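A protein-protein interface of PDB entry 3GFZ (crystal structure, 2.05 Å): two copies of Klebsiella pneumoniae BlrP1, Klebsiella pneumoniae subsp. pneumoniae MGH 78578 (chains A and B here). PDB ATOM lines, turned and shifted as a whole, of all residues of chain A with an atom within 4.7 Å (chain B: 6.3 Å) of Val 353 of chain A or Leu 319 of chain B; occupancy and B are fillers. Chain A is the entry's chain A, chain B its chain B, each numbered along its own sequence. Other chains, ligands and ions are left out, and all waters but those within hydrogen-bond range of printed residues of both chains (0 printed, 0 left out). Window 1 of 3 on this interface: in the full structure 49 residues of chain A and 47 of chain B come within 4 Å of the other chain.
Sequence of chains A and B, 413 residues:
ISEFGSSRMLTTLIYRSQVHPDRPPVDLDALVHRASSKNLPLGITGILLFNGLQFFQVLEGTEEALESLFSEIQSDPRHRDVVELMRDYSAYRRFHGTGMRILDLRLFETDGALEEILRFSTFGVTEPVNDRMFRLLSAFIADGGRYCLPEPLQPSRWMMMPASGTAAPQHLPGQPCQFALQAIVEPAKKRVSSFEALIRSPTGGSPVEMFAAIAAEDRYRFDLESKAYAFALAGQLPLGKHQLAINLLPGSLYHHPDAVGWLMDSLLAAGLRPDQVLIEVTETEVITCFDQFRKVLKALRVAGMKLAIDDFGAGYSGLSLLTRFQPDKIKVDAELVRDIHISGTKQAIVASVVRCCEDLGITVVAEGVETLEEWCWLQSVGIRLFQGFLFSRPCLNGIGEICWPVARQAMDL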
ATOM      1  N   PHE A 312      -2.520  11.007   7.128  1.00  0.00           N
ATOM      2  CA  PHE A 312      -1.176  11.091   6.624  1.00  0.00           C
ATOM      3  C   PHE A 312      -0.756  12.552   6.597  1.00  0.00           C
ATOM      4  O   PHE A 312      -1.433  13.377   5.987  1.00  0.00           O
ATOM      5  CB  PHE A 312      -1.117  10.494   5.230  1.00  0.00           C
ATOM      6  CG  PHE A 312       0.248  10.491   4.646  1.00  0.00           C
ATOM      7  CD1 PHE A 312       1.114   9.457   4.919  1.00  0.00           C
ATOM      8  CD2 PHE A 312       0.675  11.530   3.823  1.00  0.00           C
ATOM      9  CE1 PHE A 312       2.377   9.438   4.379  1.00  0.00           C
ATOM     10  CE2 PHE A 312       1.948  11.522   3.285  1.00  0.00           C
ATOM     11  CZ  PHE A 312       2.797  10.475   3.558  1.00  0.00           C
ATOM     12  N   SER A 317       5.027  12.271   9.501  1.00  0.00           N
ATOM     13  CA  SER A 317       4.757  11.775   8.157  1.00  0.00           C
ATOM     14  C   SER A 317       5.768  10.874   7.456  1.00  0.00           C
ATOM     15  O   SER A 317       6.707  10.356   8.067  1.00  0.00           O
ATOM     16  CB  SER A 317       4.182  12.895   7.273  1.00  0.00           C
ATOM     17  OG  SER A 317       5.175  13.695   6.665  1.00  0.00           O
ATOM     18  N   LEU A 319       7.507   9.794   4.150  1.00  0.00           N
ATOM     19  CA  LEU A 319       8.721   9.432   3.382  1.00  0.00           C
ATOM     20  C   LEU A 319       9.525   8.274   3.998  1.00  0.00           C
ATOM     21  O   LEU A 319      10.126   7.467   3.282  1.00  0.00           O
ATOM     22  CB  LEU A 319       9.635  10.653   3.230  1.00  0.00           C
ATOM     23  CG  LEU A 319       9.026  11.940   2.633  1.00  0.00           C
ATOM     24  CD1 LEU A 319       9.332  13.122   3.526  1.00  0.00           C
ATOM     25  CD2 LEU A 319       9.435  12.213   1.185  1.00  0.00           C
ATOM     26  N   ILE A 330      -3.505   6.463   0.682  1.00  0.00           N
ATOM     27  CA  ILE A 330      -3.162   7.402   1.755  1.00  0.00           C
ATOM     28  C   ILE A 330      -4.255   8.441   1.864  1.00  0.00           C
ATOM     29  O   ILE A 330      -4.794   8.885   0.856  1.00  0.00           O
ATOM     30  CB  ILE A 330      -1.766   8.058   1.632  1.00  0.00           C
ATOM     31  CG1 ILE A 330      -1.675   8.982   0.432  1.00  0.00           C
ATOM     32  CG2 ILE A 330      -0.665   7.002   1.551  1.00  0.00           C
ATOM     33  CD1 ILE A 330      -0.570   9.940   0.557  1.00  0.00           C
ATOM     34  N   VAL A 332      -4.924  12.123   3.142  1.00  0.00           N
ATOM     35  CA  VAL A 332      -4.218  13.349   3.507  1.00  0.00           C
ATOM     36  C   VAL A 332      -4.943  14.012   4.672  1.00  0.00           C
ATOM     37  O   VAL A 332      -6.149  14.217   4.634  1.00  0.00           O
ATOM     38  CB  VAL A 332      -4.107  14.321   2.303  1.00  0.00           C
ATOM     39  CG1 VAL A 332      -3.532  15.680   2.726  1.00  0.00           C
ATOM     40  CG2 VAL A 332      -3.257  13.695   1.195  1.00  0.00           C
ATOM     41  N   ILE A 349       3.209  20.808  -0.436  1.00  0.00           N
ATOM     42  CA  ILE A 349       3.281  19.492   0.213  1.00  0.00           C
ATOM     43  C   ILE A 349       2.255  18.532  -0.384  1.00  0.00           C
ATOM     44  O   ILE A 349       2.591  17.399  -0.751  1.00  0.00           O
ATOM     45  CB  ILE A 349       3.074  19.591   1.755  1.00  0.00           C
ATOM     46  CG1 ILE A 349       4.246  20.333   2.412  1.00  0.00           C
ATOM     47  CG2 ILE A 349       2.965  18.209   2.373  1.00  0.00           C
ATOM     48  CD1 ILE A 349       3.939  20.909   3.770  1.00  0.00           C
ATOM     49  N   VAL A 350       1.009  18.984  -0.493  1.00  0.00           N
ATOM     50  CA  VAL A 350      -0.044  18.127  -1.014  1.00  0.00           C
ATOM     51  C   VAL A 350       0.223  17.764  -2.480  1.00  0.00           C
ATOM     52  O   VAL A 350       0.053  16.621  -2.874  1.00  0.00           O
ATOM     53  CB  VAL A 350      -1.444  18.750  -0.858  1.00  0.00           C
ATOM     54  CG1 VAL A 350      -2.474  17.855  -1.491  1.00  0.00           C
ATOM     55  CG2 VAL A 350      -1.793  18.957   0.619  1.00  0.00           C
ATOM     56  N   ALA A 351       0.647  18.730  -3.278  1.00  0.00           N
ATOM     57  CA  ALA A 351       0.982  18.465  -4.675  1.00  0.00           C
ATOM     58  C   ALA A 351       2.065  17.384  -4.797  1.00  0.00           C
ATOM     59  O   ALA A 351       2.016  16.538  -5.692  1.00  0.00           O
ATOM     60  CB  ALA A 351       1.435  19.751  -5.349  1.00  0.00           C
ATOM     61  N   SER A 352       3.028  17.407  -3.884  1.00  0.00           N
ATOM     62  CA  SER A 352       4.147  16.463  -3.911  1.00  0.00           C
ATOM     63  C   SER A 352       3.699  15.055  -3.508  1.00  0.00           C
ATOM     64  O   SER A 352       4.144  14.063  -4.078  1.00  0.00           O
ATOM     65  CB  SER A 352       5.272  16.951  -2.991  1.00  0.00           C
ATOM     66  OG  SER A 352       4.985  16.654  -1.638  1.00  0.00           O
ATOM     67  N   VAL A 353       2.816  14.982  -2.520  1.00  0.00           N
ATOM     68  CA  VAL A 353       2.253  13.708  -2.063  1.00  0.00           C
ATOM     69  C   VAL A 353       1.425  13.051  -3.185  1.00  0.00           C
ATOM     70  O   VAL A 353       1.515  11.839  -3.435  1.00  0.00           O
ATOM     71  CB  VAL A 353       1.372  13.939  -0.819  1.00  0.00           C
ATOM     72  CG1 VAL A 353       0.563  12.734  -0.501  1.00  0.00           C
ATOM     73  CG2 VAL A 353       2.225  14.317   0.381  1.00  0.00           C
ATOM     74  N   VAL A 354       0.613  13.867  -3.848  1.00  0.00           N
ATOM     75  CA  VAL A 354      -0.177  13.422  -4.993  1.00  0.00           C
ATOM     76  C   VAL A 354       0.709  12.841  -6.086  1.00  0.00           C
ATOM     77  O   VAL A 354       0.398  11.787  -6.637  1.00  0.00           O
ATOM     78  CB  VAL A 354      -1.053  14.573  -5.536  1.00  0.00           C
ATOM     79  CG1 VAL A 354      -1.644  14.247  -6.900  1.00  0.00           C
ATOM     80  CG2 VAL A 354      -2.163  14.883  -4.545  1.00  0.00           C
ATOM     81  N   ARG A 355       1.815  13.512  -6.390  1.00  0.00           N
ATOM     82  CA  ARG A 355       2.699  13.058  -7.461  1.00  0.00           C
ATOM     83  C   ARG A 355       3.405  11.763  -7.081  1.00  0.00           C
ATOM     84  O   ARG A 355       3.536  10.860  -7.899  1.00  0.00           O
ATOM     85  CB  ARG A 355       3.728  14.131  -7.820  1.00  0.00           C
ATOM     86  CG  ARG A 355       4.472  13.875  -9.133  1.00  0.00           C
ATOM     87  CD  ARG A 355       3.533  13.898 -10.334  1.00  0.00           C
ATOM     88  NE  ARG A 355       4.170  14.498 -11.506  1.00  0.00           N
ATOM     89  CZ  ARG A 355       3.525  15.000 -12.564  1.00  0.00           C
ATOM     90  NH1 ARG A 355       2.193  14.978 -12.646  1.00  0.00           N
ATOM     91  NH2 ARG A 355       4.224  15.535 -13.560  1.00  0.00           N
ATOM     92  N   CYS A 356       3.840  11.675  -5.827  1.00  0.00           N
ATOM     93  CA  CYS A 356       4.539  10.493  -5.339  1.00  0.00           C
ATOM     94  C   CYS A 356       3.623   9.261  -5.373  1.00  0.00           C
ATOM     95  O   CYS A 356       3.989   8.219  -5.903  1.00  0.00           O
ATOM     96  CB  CYS A 356       5.053  10.750  -3.919  1.00  0.00           C
ATOM     97  SG  CYS A 356       6.143   9.498  -3.304  1.00  0.00           S
ATOM     98  N   CYS A 357       2.420   9.405  -4.823  1.00  0.00           N
ATOM     99  CA  CYS A 357       1.407   8.346  -4.848  1.00  0.00           C
ATOM    100  C   CYS A 357       1.025   7.896  -6.250  1.00  0.00           C
ATOM    101  O   CYS A 357       0.850   6.708  -6.497  1.00  0.00           O
ATOM    102  CB  CYS A 357       0.154   8.825  -4.131  1.00  0.00           C
ATOM    103  SG  CYS A 357       0.423   9.003  -2.399  1.00  0.00           S
ATOM    104  N   VAL A 364      -4.995   8.470  -3.479  1.00  0.00           N
ATOM    105  CA  VAL A 364      -4.984   9.575  -2.516  1.00  0.00           C
ATOM    106  C   VAL A 364      -6.387  10.160  -2.274  1.00  0.00           C
ATOM    107  O   VAL A 364      -7.091  10.510  -3.215  1.00  0.00           O
ATOM    108  CB  VAL A 364      -4.021  10.694  -2.937  1.00  0.00           C
ATOM    109  CG1 VAL A 364      -4.040  11.838  -1.924  1.00  0.00           C
ATOM    110  CG2 VAL A 364      -2.615  10.146  -3.046  1.00  0.00           C
ATOM    111  N   GLU B 283      16.252  15.422  11.448  1.00  0.00           N
ATOM    112  CA  GLU B 283      14.807  15.546  11.722  1.00  0.00           C
ATOM    113  C   GLU B 283      14.387  14.717  12.925  1.00  0.00           C
ATOM    114  O   GLU B 283      13.528  15.146  13.682  1.00  0.00           O
ATOM    115  CB  GLU B 283      13.908  15.179  10.530  1.00  0.00           C
ATOM    116  CG  GLU B 283      12.424  15.549  10.803  1.00  0.00           C
ATOM    117  CD  GLU B 283      11.489  15.345   9.623  1.00  0.00           C
ATOM    118  OE1 GLU B 283      11.795  15.836   8.519  1.00  0.00           O
ATOM    119  OE2 GLU B 283      10.422  14.717   9.812  1.00  0.00           O
ATOM    120  N   PHE B 312      17.392  13.636   6.061  1.00  0.00           N
ATOM    121  CA  PHE B 312      15.986  13.681   5.714  1.00  0.00           C
ATOM    122  C   PHE B 312      15.615  12.397   4.973  1.00  0.00           C
ATOM    123  O   PHE B 312      16.141  12.111   3.911  1.00  0.00           O
ATOM    124  CB  PHE B 312      15.674  14.901   4.849  1.00  0.00           C
ATOM    125  CG  PHE B 312      14.202  15.146   4.664  1.00  0.00           C
ATOM    126  CD1 PHE B 312      13.471  15.841   5.618  1.00  0.00           C
ATOM    127  CD2 PHE B 312      13.546  14.680   3.544  1.00  0.00           C
ATOM    128  CE1 PHE B 312      12.116  16.071   5.445  1.00  0.00           C
ATOM    129  CE2 PHE B 312      12.192  14.911   3.367  1.00  0.00           C
ATOM    130  CZ  PHE B 312      11.479  15.602   4.317  1.00  0.00           C
ATOM    131  N   SER B 317      10.543  11.080   8.900  1.00  0.00           N
ATOM    132  CA  SER B 317      10.864  12.112   7.921  1.00  0.00           C
ATOM    133  C   SER B 317       9.619  12.556   7.195  1.00  0.00           C
ATOM    134  O   SER B 317       8.886  11.724   6.658  1.00  0.00           O
ATOM    135  CB  SER B 317      11.866  11.569   6.928  1.00  0.00           C
ATOM    136  OG  SER B 317      13.151  11.542   7.529  1.00  0.00           O
ATOM    137  N   GLY B 318       9.392  13.866   7.157  1.00  0.00           N
ATOM    138  CA  GLY B 318       8.108  14.387   6.734  1.00  0.00           C
ATOM    139  C   GLY B 318       8.106  15.736   6.066  1.00  0.00           C
ATOM    140  O   GLY B 318       8.877  16.628   6.416  1.00  0.00           O
ATOM    141  N   LEU B 319       7.203  15.866   5.103  1.00  0.00           N
ATOM    142  CA  LEU B 319       6.927  17.124   4.439  1.00  0.00           C
ATOM    143  C   LEU B 319       6.091  17.994   5.371  1.00  0.00           C
ATOM    144  O   LEU B 319       6.158  19.214   5.304  1.00  0.00           O
ATOM    145  CB  LEU B 319       6.154  16.862   3.146  1.00  0.00           C
ATOM    146  CG  LEU B 319       6.790  15.881   2.148  1.00  0.00           C
ATOM    147  CD1 LEU B 319       5.772  14.833   1.689  1.00  0.00           C
ATOM    148  CD2 LEU B 319       7.408  16.602   0.961  1.00  0.00           C
ATOM    149  N   SER B 320       5.309  17.351   6.240  1.00  0.00           N
ATOM    150  CA  SER B 320       4.509  18.020   7.270  1.00  0.00           C
ATOM    151  C   SER B 320       5.339  18.793   8.292  1.00  0.00           C
ATOM    152  O   SER B 320       4.850  19.741   8.909  1.00  0.00           O
ATOM    153  CB  SER B 320       3.723  16.958   8.008  1.00  0.00           C
ATOM    154  OG  SER B 320       4.538  15.811   8.130  1.00  0.00           O
ATOM    155  N   LEU B 321       6.580  18.350   8.495  1.00  0.00           N
ATOM    156  CA  LEU B 321       7.599  19.136   9.196  1.00  0.00           C
ATOM    157  C   LEU B 321       7.652  20.565   8.630  1.00  0.00           C
ATOM    158  O   LEU B 321       7.813  21.530   9.380  1.00  0.00           O
ATOM    159  CB  LEU B 321       8.965  18.444   9.037  1.00  0.00           C
ATOM    160  CG  LEU B 321      10.238  18.878   9.778  1.00  0.00           C
ATOM    161  CD1 LEU B 321      10.867  20.135   9.179  1.00  0.00           C
ATOM    162  CD2 LEU B 321       9.997  19.053  11.264  1.00  0.00           C
ATOM    163  N   LEU B 322       7.481  20.684   7.312  1.00  0.00           N
ATOM    164  CA  LEU B 322       7.642  21.949   6.598  1.00  0.00           C
ATOM    165  C   LEU B 322       6.552  22.983   6.865  1.00  0.00           C
ATOM    166  O   LEU B 322       6.787  24.168   6.665  1.00  0.00           O
ATOM    167  CB  LEU B 322       7.768  21.711   5.091  1.00  0.00           C
ATOM    168  CG  LEU B 322       8.926  20.784   4.694  1.00  0.00           C
ATOM    169  CD1 LEU B 322       8.719  20.123   3.332  1.00  0.00           C
ATOM    170  CD2 LEU B 322      10.240  21.552   4.735  1.00  0.00           C
ATOM    171  N   THR B 323       5.369  22.546   7.300  1.00  0.00           N
ATOM    172  CA  THR B 323       4.283  23.473   7.635  1.00  0.00           C
ATOM    173  C   THR B 323       4.577  24.273   8.903  1.00  0.00           C
ATOM    174  O   THR B 323       4.142  25.419   9.032  1.00  0.00           O
ATOM    175  CB  THR B 323       2.940  22.737   7.842  1.00  0.00           C
ATOM    176  OG1 THR B 323       3.138  21.603   8.701  1.00  0.00           O
ATOM    177  CG2 THR B 323       2.361  22.276   6.514  1.00  0.00           C
ATOM    178  N   SER B 352       9.829  13.619  -5.547  1.00  0.00           N
ATOM    179  CA  SER B 352       8.833  14.380  -4.812  1.00  0.00           C
ATOM    180  C   SER B 352       9.450  15.367  -3.816  1.00  0.00           C
ATOM    181  O   SER B 352       8.964  16.486  -3.682  1.00  0.00           O
ATOM    182  CB  SER B 352       7.893  13.432  -4.071  1.00  0.00           C
ATOM    183  OG  SER B 352       6.769  14.147  -3.596  1.00  0.00           O
ATOM    184  N   VAL B 353      10.496  14.941  -3.106  1.00  0.00           N
ATOM    185  CA  VAL B 353      11.239  15.844  -2.212  1.00  0.00           C
ATOM    186  C   VAL B 353      11.850  17.008  -3.006  1.00  0.00           C
ATOM    187  O   VAL B 353      11.741  18.171  -2.603  1.00  0.00           O
ATOM    188  CB  VAL B 353      12.353  15.103  -1.434  1.00  0.00           C
ATOM    189  CG1 VAL B 353      13.285  16.089  -0.725  1.00  0.00           C
ATOM    190  CG2 VAL B 353      11.748  14.116  -0.421  1.00  0.00           C
ATOM    191  N   CYS B 356       9.091  19.468  -4.161  1.00  0.00           N
ATOM    192  CA  CYS B 356       8.533  20.193  -3.028  1.00  0.00           C
ATOM    193  C   CYS B 356       9.486  21.283  -2.549  1.00  0.00           C
ATOM    194  O   CYS B 356       9.072  22.405  -2.282  1.00  0.00           O
ATOM    195  CB  CYS B 356       8.223  19.241  -1.874  1.00  0.00           C
ATOM    196  SG  CYS B 356       7.239  20.015  -0.591  1.00  0.00           S
ATOM    197  N   LEU B 360       9.104  25.335  -2.385  1.00  0.00           N
ATOM    198  CA  LEU B 360       9.290  25.988  -1.094  1.00  0.00           C
ATOM    199  C   LEU B 360      10.553  26.856  -1.016  1.00  0.00           C
ATOM    200  O   LEU B 360      10.713  27.597  -0.056  1.00  0.00           O
ATOM    201  CB  LEU B 360       9.332  24.950   0.031  1.00  0.00           C
ATOM    202  CG  LEU B 360       8.090  24.104   0.327  1.00  0.00           C
ATOM    203  CD1 LEU B 360       8.412  23.098   1.405  1.00  0.00           C
ATOM    204  CD2 LEU B 360       6.937  24.948   0.751  1.00  0.00           C
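Among the printed residues, merely in contact across the chains: Ser 317 of chain A with Gly 318 of chain B (3.0 Å), Leu 319 of chain A with Phe 312 of chain B (3.4 Å), Leu 319 of chain A with Gly 318 of chain B (3.7 Å), Leu 319 of chain A with Leu 319 of chain B (3.8 Å), Leu 319 of chain A with Val 353 of chain B (3.4 Å), Ile 349 of chain A with Leu 319 of chain B (3.2 Å), Ile 349 of chain A with Thr 323 of chain B (3.4 Å), Ser 352 of chain A with Leu 319 of chain B (3.6 Å), Ser 352 of chain A with Cys 356 of chain B (3.9 Å), Val 353 of chain A with Leu 319 of chain B (3.8 Å) and Cys 356 of chain A with Ser 352 of chain B (3.8 Å).
Printed residues of chain B within 4 Å of Ile 349 of chain A: Leu 319 and Thr 323. Val 354 of chain A touches none of the printed residues of chain B. Printed residues of chain A within 4 Å of Ser 317 of chain B: Ser 317 and Leu 319. Leu 319 of chain B touches just these residues of chain A: Ser 317 (3.4 Å), Leu 319 (3.8 Å), Ile 349 (3.2 Å), Ser 352 (3.6 Å) and Val 353 (3.8 Å). Printed residues of chain A within 4 Å of Ser 352 of chain B: Ser 352 and Cys 356. The nearest printed residue of chain A that does not touch Leu 319 of chain B is Phe 312 of chain A (5.3 Å). The nearest printed residue of chain A that does not touch Gly 318 of chain B is Ile 349 of chain A (6.8 Å).
The backbone NH (N) of Gly 318 of chain B is in hydrogen-bond range of the side-chain carboxylate (OE2) of Glu 283 of chain B, 3.0 Å away. OG of Ser 352 of chain A lies within hydrogen-bond range of O of Ile 349 of chain A (2.7 Å). O of Ser 320 of chain B lies within hydrogen-bond range of OG1 of Thr 323 of chain B (2.5 Å). The backbone carbonyl oxygen (O) of Val 353 of chain A lies within hydrogen-bond range of the side-chain sulfur (SG) of Cys 357 of chain A, at 3.2 Å.
The backbone carbonyl oxygen (O) of Ser 352 of chain A lies within hydrogen-bond range of the side-chain hydroxyl (OG) of Ser 352 of chain B (2.7 Å). The backbone carbonyl oxygen (O) of Ser 317 of chain B is in hydrogen-bond range of the backbone NH (N) of Leu 319 of chain A (3.5 Å). O of Ser 317 of chain A sits close to O of Ser 317 of chain B, 2.9 Å away. The side-chain hydroxyl (OG) of Ser 317 of chain A lies within hydrogen-bond range of the backbone NH (N) of Leu 319 of chain B. The side-chain hydroxyl (OG) of Ser 320 of chain B sits at hydrogen-bond distance from the side-chain hydroxyl (OG) of Ser 317 of chain A.
Of the 15 printed residues of chain A, 6 touch a printed residue of chain B. Hydrophobic or aromatic side chains of chain A within 4 Å of the printed part of chain B: Leu 319, Ile 349 and Val 353. Among the printed residues, no Asp or Glu carboxylate lies within 4 Å of a Lys or Arg side-chain nitrogen of the other chain.
Ser 317 of chain A touches its own counterpart, Ser 317 of chain B. Ser 317 of chain A touches Leu 319 of chain B, and with the chains exchanged Leu 319 of chain A touches Ser 317 of chain B. Leu 319 of chain A touches Val 353 of chain B, and with the chains exchanged Val 353 of chain A touches Leu 319 of chain B. Ser 352 of chain A touches Leu 319 of chain B, but with the chains exchanged Leu 319 of chain A does not touch Ser 352 of chain B (5.6 Å). Positions printed for both chains: 312, 317, 319, 352, 353 and 356.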
